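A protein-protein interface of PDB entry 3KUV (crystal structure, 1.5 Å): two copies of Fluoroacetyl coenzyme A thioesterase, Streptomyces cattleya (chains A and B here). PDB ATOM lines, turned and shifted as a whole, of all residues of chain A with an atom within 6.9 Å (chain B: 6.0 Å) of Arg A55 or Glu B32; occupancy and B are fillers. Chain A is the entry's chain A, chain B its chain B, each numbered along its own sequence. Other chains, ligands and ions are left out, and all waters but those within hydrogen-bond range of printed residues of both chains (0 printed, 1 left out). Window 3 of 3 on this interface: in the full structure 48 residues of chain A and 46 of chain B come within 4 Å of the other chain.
The indole nitrogen (NE1) of Trp A51 lies within hydrogen-bond range of the side-chain carboxylate (OE2) of Glu B32, 2.8 Å away.
The indole nitrogen (NE1) of Trp A51 sits at hydrogen-bond distance from the side-chain hydroxyl (OG) of Ser B30 (3.2 Å).
Glu B32 touches just these residues of chain A: Trp A51, Val A54 and Arg A55.
Of the printed residues of chain A, Ser B30 touches Trp A51 (3.2 Å).
Printed residues of chain B within 4 Å of Val A54: Glu B32 and Phe B36.
Of the printed residues of chain B, Trp A51 touches Ser B30 (3.2 Å), Glu B32 (2.8 Å) and Phe B33 (3.5 Å).
Of the printed residues of chain A, Phe B36 touches Val A54 (3.99 Å).
The nearest printed residue of chain A that does not touch Ser B30 is Val A54 (6.5 Å).
NH1 of Arg A55 is in hydrogen-bond range of ND1 of His A13 (2.8 Å).
The side-chain hydroxyl (OG) of Ser B30 sits at hydrogen-bond distance from the backbone NH (N) of Phe B33.
OG of Ser B30 sits close to N of Glu B32 (3.2 Å).
No position is printed for both chains.
Of the 6 pairs that touch across the chains among the printed residues, none has its exchanged pair printed and touching as well.
Hydrophobic or aromatic side chains of chain B within 4 Å of the printed part of chain A: Phe B33 and Phe B36.
Printed residues of chain A that touch a printed residue of chain B: Trp A51, Val A54 and Arg A55.
Hydrophobic or aromatic side chains of chain A that line the printed part of chain B: Trp A51 and Val A54.
Among the printed residues, 6 pairs touch across the chains.
Among the printed residues, pairs that only touch across the chains: Trp A51 with Phe B33, Arg A55 with Glu B32, Val A54 with Glu B32 and Val A54 with Phe B36.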
ATOM      1  N   PHE A  11      -6.827   9.900  28.261  1.00  0.00           N
ATOM      2  CA  PHE A  11      -7.659  10.030  27.046  1.00  0.00           C
ATOM      3  C   PHE A  11      -8.095  11.498  27.051  1.00  0.00           C
ATOM      4  O   PHE A  11      -8.522  11.990  28.076  1.00  0.00           O
ATOM      5  CB  PHE A  11      -8.871   9.201  27.113  1.00  0.00           C
ATOM      6  CG  PHE A  11      -9.789   9.364  25.925  1.00  0.00           C
ATOM      7  CD1 PHE A  11      -9.534   8.651  24.726  1.00  0.00           C
ATOM      8  CD2 PHE A  11     -10.890  10.214  25.951  1.00  0.00           C
ATOM      9  CE1 PHE A  11     -10.415   8.853  23.597  1.00  0.00           C
ATOM     10  CE2 PHE A  11     -11.730  10.447  24.807  1.00  0.00           C
ATOM     11  CZ  PHE A  11     -11.481   9.725  23.638  1.00  0.00           C
ATOM     12  N   THR A  12      -8.079  12.174  25.912  1.00  0.00           N
ATOM     13  CA  THR A  12      -8.487  13.568  25.846  1.00  0.00           C
ATOM     14  C   THR A  12      -9.575  13.767  24.876  1.00  0.00           C
ATOM     15  O   THR A  12      -9.667  13.071  23.845  1.00  0.00           O
ATOM     16  CB  THR A  12      -7.352  14.524  25.651  1.00  0.00           C
ATOM     17  OG1 THR A  12      -6.959  14.549  24.282  1.00  0.00           O
ATOM     18  CG2 THR A  12      -6.257  14.081  26.550  1.00  0.00           C
ATOM     19  N   HIS A  13     -10.431  14.780  25.190  1.00  0.00           N
ATOM     20  CA  HIS A  13     -11.580  15.076  24.428  1.00  0.00           C
ATOM     21  C   HIS A  13     -11.794  16.604  24.389  1.00  0.00           C
ATOM     22  O   HIS A  13     -11.809  17.212  25.455  1.00  0.00           O
ATOM     23  CB  HIS A  13     -12.731  14.376  25.262  1.00  0.00           C
ATOM     24  CG  HIS A  13     -14.059  14.640  24.756  1.00  0.00           C
ATOM     25  ND1 HIS A  13     -14.645  13.789  23.848  1.00  0.00           N
ATOM     26  CD2 HIS A  13     -15.001  15.538  25.113  1.00  0.00           C
ATOM     27  CE1 HIS A  13     -15.860  14.252  23.549  1.00  0.00           C
ATOM     28  NE2 HIS A  13     -16.110  15.301  24.319  1.00  0.00           N
ATOM     29  N   ASP A  14     -11.920  17.178  23.206  1.00  0.00           N
ATOM     30  CA  ASP A  14     -12.040  18.660  23.035  1.00  0.00           C
ATOM     31  C   ASP A  14     -13.414  19.085  22.602  1.00  0.00           C
ATOM     32  O   ASP A  14     -14.082  18.376  21.811  1.00  0.00           O
ATOM     33  CB  ASP A  14     -11.043  19.203  21.983  1.00  0.00           C
ATOM     34  CG  ASP A  14      -9.641  18.718  22.208  1.00  0.00           C
ATOM     35  OD1 ASP A  14      -9.090  18.860  23.338  1.00  0.00           O
ATOM     36  OD2 ASP A  14      -8.981  18.194  21.275  1.00  0.00           O
ATOM     37  N   GLU A  50     -18.048  13.091  31.751  1.00  0.00           N
ATOM     38  CA  GLU A  50     -18.568  11.714  31.694  1.00  0.00           C
ATOM     39  C   GLU A  50     -18.505  11.205  30.209  1.00  0.00           C
ATOM     40  O   GLU A  50     -18.106  10.050  29.977  1.00  0.00           O
ATOM     41  CB  GLU A  50     -19.989  11.679  32.335  1.00  0.00           C
ATOM     42  CG  GLU A  50     -19.931  12.051  33.817  1.00  0.00           C
ATOM     43  CD  GLU A  50     -21.300  12.007  34.509  1.00  0.00           C
ATOM     44  OE1 GLU A  50     -22.317  11.788  33.832  1.00  0.00           O
ATOM     45  OE2 GLU A  50     -21.331  12.176  35.759  1.00  0.00           O
ATOM     46  N   TRP A  51     -18.849  12.068  29.273  1.00  0.00           N
ATOM     47  CA  TRP A  51     -18.704  11.717  27.850  1.00  0.00           C
ATOM     48  C   TRP A  51     -17.251  11.285  27.487  1.00  0.00           C
ATOM     49  O   TRP A  51     -17.042  10.266  26.754  1.00  0.00           O
ATOM     50  CB  TRP A  51     -19.145  12.937  27.028  1.00  0.00           C
ATOM     51  CG  TRP A  51     -19.218  12.690  25.494  1.00  0.00           C
ATOM     52  CD1 TRP A  51     -19.094  11.504  24.812  1.00  0.00           C
ATOM     53  CD2 TRP A  51     -19.462  13.701  24.559  1.00  0.00           C
ATOM     54  NE1 TRP A  51     -19.201  11.784  23.414  1.00  0.00           N
ATOM     55  CE2 TRP A  51     -19.470  13.111  23.250  1.00  0.00           C
ATOM     56  CE3 TRP A  51     -19.717  15.080  24.684  1.00  0.00           C
ATOM     57  CZ2 TRP A  51     -19.637  13.882  22.076  1.00  0.00           C
ATOM     58  CZ3 TRP A  51     -19.896  15.895  23.494  1.00  0.00           C
ATOM     59  CH2 TRP A  51     -19.849  15.257  22.184  1.00  0.00           C
ATOM     60  N   ALA A  52     -16.262  12.027  28.006  1.00  0.00           N
ATOM     61  CA  ALA A  52     -14.835  11.632  27.743  1.00  0.00           C
ATOM     62  C   ALA A  52     -14.578  10.207  28.250  1.00  0.00           C
ATOM     63  O   ALA A  52     -13.934   9.357  27.610  1.00  0.00           O
ATOM     64  CB  ALA A  52     -13.875  12.597  28.347  1.00  0.00           C
ATOM     65  N   CYS A  53     -15.109   9.895  29.456  1.00  0.00           N
ATOM     66  CA  CYS A  53     -14.845   8.588  30.052  1.00  0.00           C
ATOM     67  C   CYS A  53     -15.613   7.475  29.320  1.00  0.00           C
ATOM     68  O   CYS A  53     -15.096   6.376  29.138  1.00  0.00           O
ATOM     69  CB  CYS A  53     -15.280   8.577  31.519  1.00  0.00           C
ATOM     70  SG  CYS A  53     -14.285   9.644  32.592  1.00  0.00           S
ATOM     71  N   VAL A  54     -16.837   7.762  28.846  1.00  0.00           N
ATOM     72  CA  VAL A  54     -17.564   6.796  28.020  1.00  0.00           C
ATOM     73  C   VAL A  54     -16.774   6.484  26.730  1.00  0.00           C
ATOM     74  O   VAL A  54     -16.726   5.282  26.413  1.00  0.00           O
ATOM     75  CB  VAL A  54     -18.958   7.409  27.663  1.00  0.00           C
ATOM     76  CG1 VAL A  54     -19.601   6.659  26.484  1.00  0.00           C
ATOM     77  CG2 VAL A  54     -19.877   7.416  28.868  1.00  0.00           C
ATOM     78  N   ARG A  55     -16.215   7.466  26.052  1.00  0.00           N
ATOM     79  CA  ARG A  55     -15.423   7.204  24.791  1.00  0.00           C
ATOM     80  C   ARG A  55     -14.176   6.414  25.203  1.00  0.00           C
ATOM     81  O   ARG A  55     -13.796   5.453  24.516  1.00  0.00           O
ATOM     82  CB  ARG A  55     -14.984   8.501  24.187  1.00  0.00           C
ATOM     83  CG  ARG A  55     -16.229   9.181  23.492  1.00  0.00           C
ATOM     84  CD  ARG A  55     -15.909  10.386  22.826  1.00  0.00           C
ATOM     85  NE  ARG A  55     -14.981  10.175  21.669  1.00  0.00           N
ATOM     86  CZ  ARG A  55     -14.465  11.153  20.998  1.00  0.00           C
ATOM     87  NH1 ARG A  55     -14.658  12.421  21.384  1.00  0.00           N
ATOM     88  NH2 ARG A  55     -13.760  10.885  19.879  1.00  0.00           N
ATOM     89  N   ALA A  56     -13.588   6.723  26.352  1.00  0.00           N
ATOM     90  CA  ALA A  56     -12.336   5.999  26.782  1.00  0.00           C
ATOM     91  C   ALA A  56     -12.605   4.528  27.086  1.00  0.00           C
ATOM     92  O   ALA A  56     -11.700   3.670  26.842  1.00  0.00           O
ATOM     93  CB  ALA A  56     -11.709   6.757  27.987  1.00  0.00           C
ATOM     94  N   MET A  57     -13.773   4.196  27.577  1.00  0.00           N
ATOM     95  CA  MET A  57     -14.019   2.815  27.944  1.00  0.00           C
ATOM     96  C   MET A  57     -14.743   1.967  26.895  1.00  0.00           C
ATOM     97  O   MET A  57     -15.047   0.793  27.195  1.00  0.00           O
ATOM     98  CB  MET A  57     -14.754   2.720  29.283  1.00  0.00           C
ATOM     99  CG  MET A  57     -16.213   3.269  29.250  1.00  0.00           C
ATOM    100  SD  MET A  57     -17.146   2.913  30.733  1.00  0.00           S
ATOM    101  CE  MET A  57     -17.557   1.191  30.531  1.00  0.00           C
ATOM    102  N   ALA A  58     -15.022   2.545  25.728  1.00  0.00           N
ATOM    103  CA  ALA A  58     -15.907   1.759  24.823  1.00  0.00           C
ATOM    104  C   ALA A  58     -15.321   0.354  24.393  1.00  0.00           C
ATOM    105  O   ALA A  58     -16.092  -0.612  24.371  1.00  0.00           O
ATOM    106  CB  ALA A  58     -16.263   2.536  23.637  1.00  0.00           C
ATOM    107  N   PRO A  59     -13.988   0.284  24.251  1.00  0.00           N
ATOM    108  CA  PRO A  59     -13.391  -1.106  24.001  1.00  0.00           C
ATOM    109  C   PRO A  59     -13.598  -2.161  25.048  1.00  0.00           C
ATOM    110  O   PRO A  59     -13.479  -3.367  24.826  1.00  0.00           O
ATOM    111  CB  PRO A  59     -11.914  -0.828  23.903  1.00  0.00           C
ATOM    112  CG  PRO A  59     -11.823   0.498  23.320  1.00  0.00           C
ATOM    113  CD  PRO A  59     -12.956   1.306  24.098  1.00  0.00           C
ATOM    114  N   SER B  30     -23.782  14.199  20.975  1.00  0.00           N
ATOM    115  CA  SER B  30     -22.990  13.009  21.282  1.00  0.00           C
ATOM    116  C   SER B  30     -23.674  11.812  20.736  1.00  0.00           C
ATOM    117  O   SER B  30     -24.756  11.428  21.212  1.00  0.00           O
ATOM    118  CB  SER B  30     -22.929  12.829  22.831  1.00  0.00           C
ATOM    119  OG  SER B  30     -22.367  11.543  23.111  1.00  0.00           O
ATOM    120  N   PRO B  31     -23.059  11.149  19.739  1.00  0.00           N
ATOM    121  CA  PRO B  31     -23.548   9.856  19.312  1.00  0.00           C
ATOM    122  C   PRO B  31     -23.540   8.778  20.365  1.00  0.00           C
ATOM    123  O   PRO B  31     -24.418   7.922  20.339  1.00  0.00           O
ATOM    124  CB  PRO B  31     -22.609   9.497  18.088  1.00  0.00           C
ATOM    125  CG  PRO B  31     -21.880  10.792  17.776  1.00  0.00           C
ATOM    126  CD  PRO B  31     -21.824  11.565  19.081  1.00  0.00           C
ATOM    127  N   GLU B  32     -22.604   8.892  21.317  1.00  0.00           N
ATOM    128  CA  GLU B  32     -22.569   7.885  22.369  1.00  0.00           C
ATOM    129  C   GLU B  32     -23.859   8.056  23.265  1.00  0.00           C
ATOM    130  O   GLU B  32     -24.548   7.053  23.576  1.00  0.00           O
ATOM    131  CB  GLU B  32     -21.305   8.086  23.273  1.00  0.00           C
ATOM    132  CG  GLU B  32     -20.042   7.602  22.540  1.00  0.00           C
ATOM    133  CD  GLU B  32     -19.483   8.584  21.527  1.00  0.00           C
ATOM    134  OE1 GLU B  32     -18.548   8.149  20.846  1.00  0.00           O
ATOM    135  OE2 GLU B  32     -19.759   9.785  21.503  1.00  0.00           O
ATOM    136  N   PHE B  33     -24.178   9.282  23.598  1.00  0.00           N
ATOM    137  CA  PHE B  33     -25.360   9.536  24.498  1.00  0.00           C
ATOM    138  C   PHE B  33     -26.677   9.231  23.816  1.00  0.00           C
ATOM    139  O   PHE B  33     -27.667   8.908  24.490  1.00  0.00           O
ATOM    140  CB  PHE B  33     -25.379  10.947  25.066  1.00  0.00           C
ATOM    141  CG  PHE B  33     -24.328  11.240  26.126  1.00  0.00           C
ATOM    142  CD1 PHE B  33     -24.343  12.461  26.746  1.00  0.00           C
ATOM    143  CD2 PHE B  33     -23.357  10.314  26.469  1.00  0.00           C
ATOM    144  CE1 PHE B  33     -23.412  12.830  27.772  1.00  0.00           C
ATOM    145  CE2 PHE B  33     -22.378  10.634  27.455  1.00  0.00           C
ATOM    146  CZ  PHE B  33     -22.369  11.902  28.077  1.00  0.00           C
ATOM    147  N   ALA B  34     -26.673   9.256  22.480  1.00  0.00           N
ATOM    148  CA  ALA B  34     -27.905   9.074  21.729  1.00  0.00           C
ATOM    149  C   ALA B  34     -28.467   7.676  21.866  1.00  0.00           C
ATOM    150  O   ALA B  34     -29.687   7.520  21.671  1.00  0.00           O
ATOM    151  CB  ALA B  34     -27.633   9.477  20.226  1.00  0.00           C
ATOM    152  N   GLU B  35     -27.626   6.680  22.201  1.00  0.00           N
ATOM    153  CA  GLU B  35     -28.024   5.284  22.382  1.00  0.00           C
ATOM    154  C   GLU B  35     -28.294   4.874  23.838  1.00  0.00           C
ATOM    155  O   GLU B  35     -28.539   3.687  24.124  1.00  0.00           O
ATOM    156  CB  GLU B  35     -27.012   4.301  21.773  1.00  0.00           C
ATOM    157  CG  GLU B  35     -25.581   4.363  22.281  1.00  0.00           C
ATOM    158  CD  GLU B  35     -24.613   3.323  21.586  1.00  0.00           C
ATOM    159  OE1 GLU B  35     -23.370   3.559  21.565  1.00  0.00           O
ATOM    160  OE2 GLU B  35     -25.086   2.282  21.053  1.00  0.00           O
ATOM    161  N   PHE B  36     -28.177   5.825  24.773  1.00  0.00           N
ATOM    162  CA  PHE B  36     -28.307   5.426  26.169  1.00  0.00           C
ATOM    163  C   PHE B  36     -29.763   5.198  26.557  1.00  0.00           C
ATOM    164  O   PHE B  36     -30.681   5.773  25.944  1.00  0.00           O
ATOM    165  CB  PHE B  36     -27.779   6.552  27.088  1.00  0.00           C
ATOM    166  CG  PHE B  36     -26.310   6.413  27.540  1.00  0.00           C
ATOM    167  CD1 PHE B  36     -25.991   6.398  28.895  1.00  0.00           C
ATOM    168  CD2 PHE B  36     -25.294   6.385  26.616  1.00  0.00           C
ATOM    169  CE1 PHE B  36     -24.667   6.301  29.296  1.00  0.00           C
ATOM    170  CE2 PHE B  36     -23.943   6.236  27.029  1.00  0.00           C
ATOM    171  CZ  PHE B  36     -23.660   6.260  28.377  1.00  0.00           C
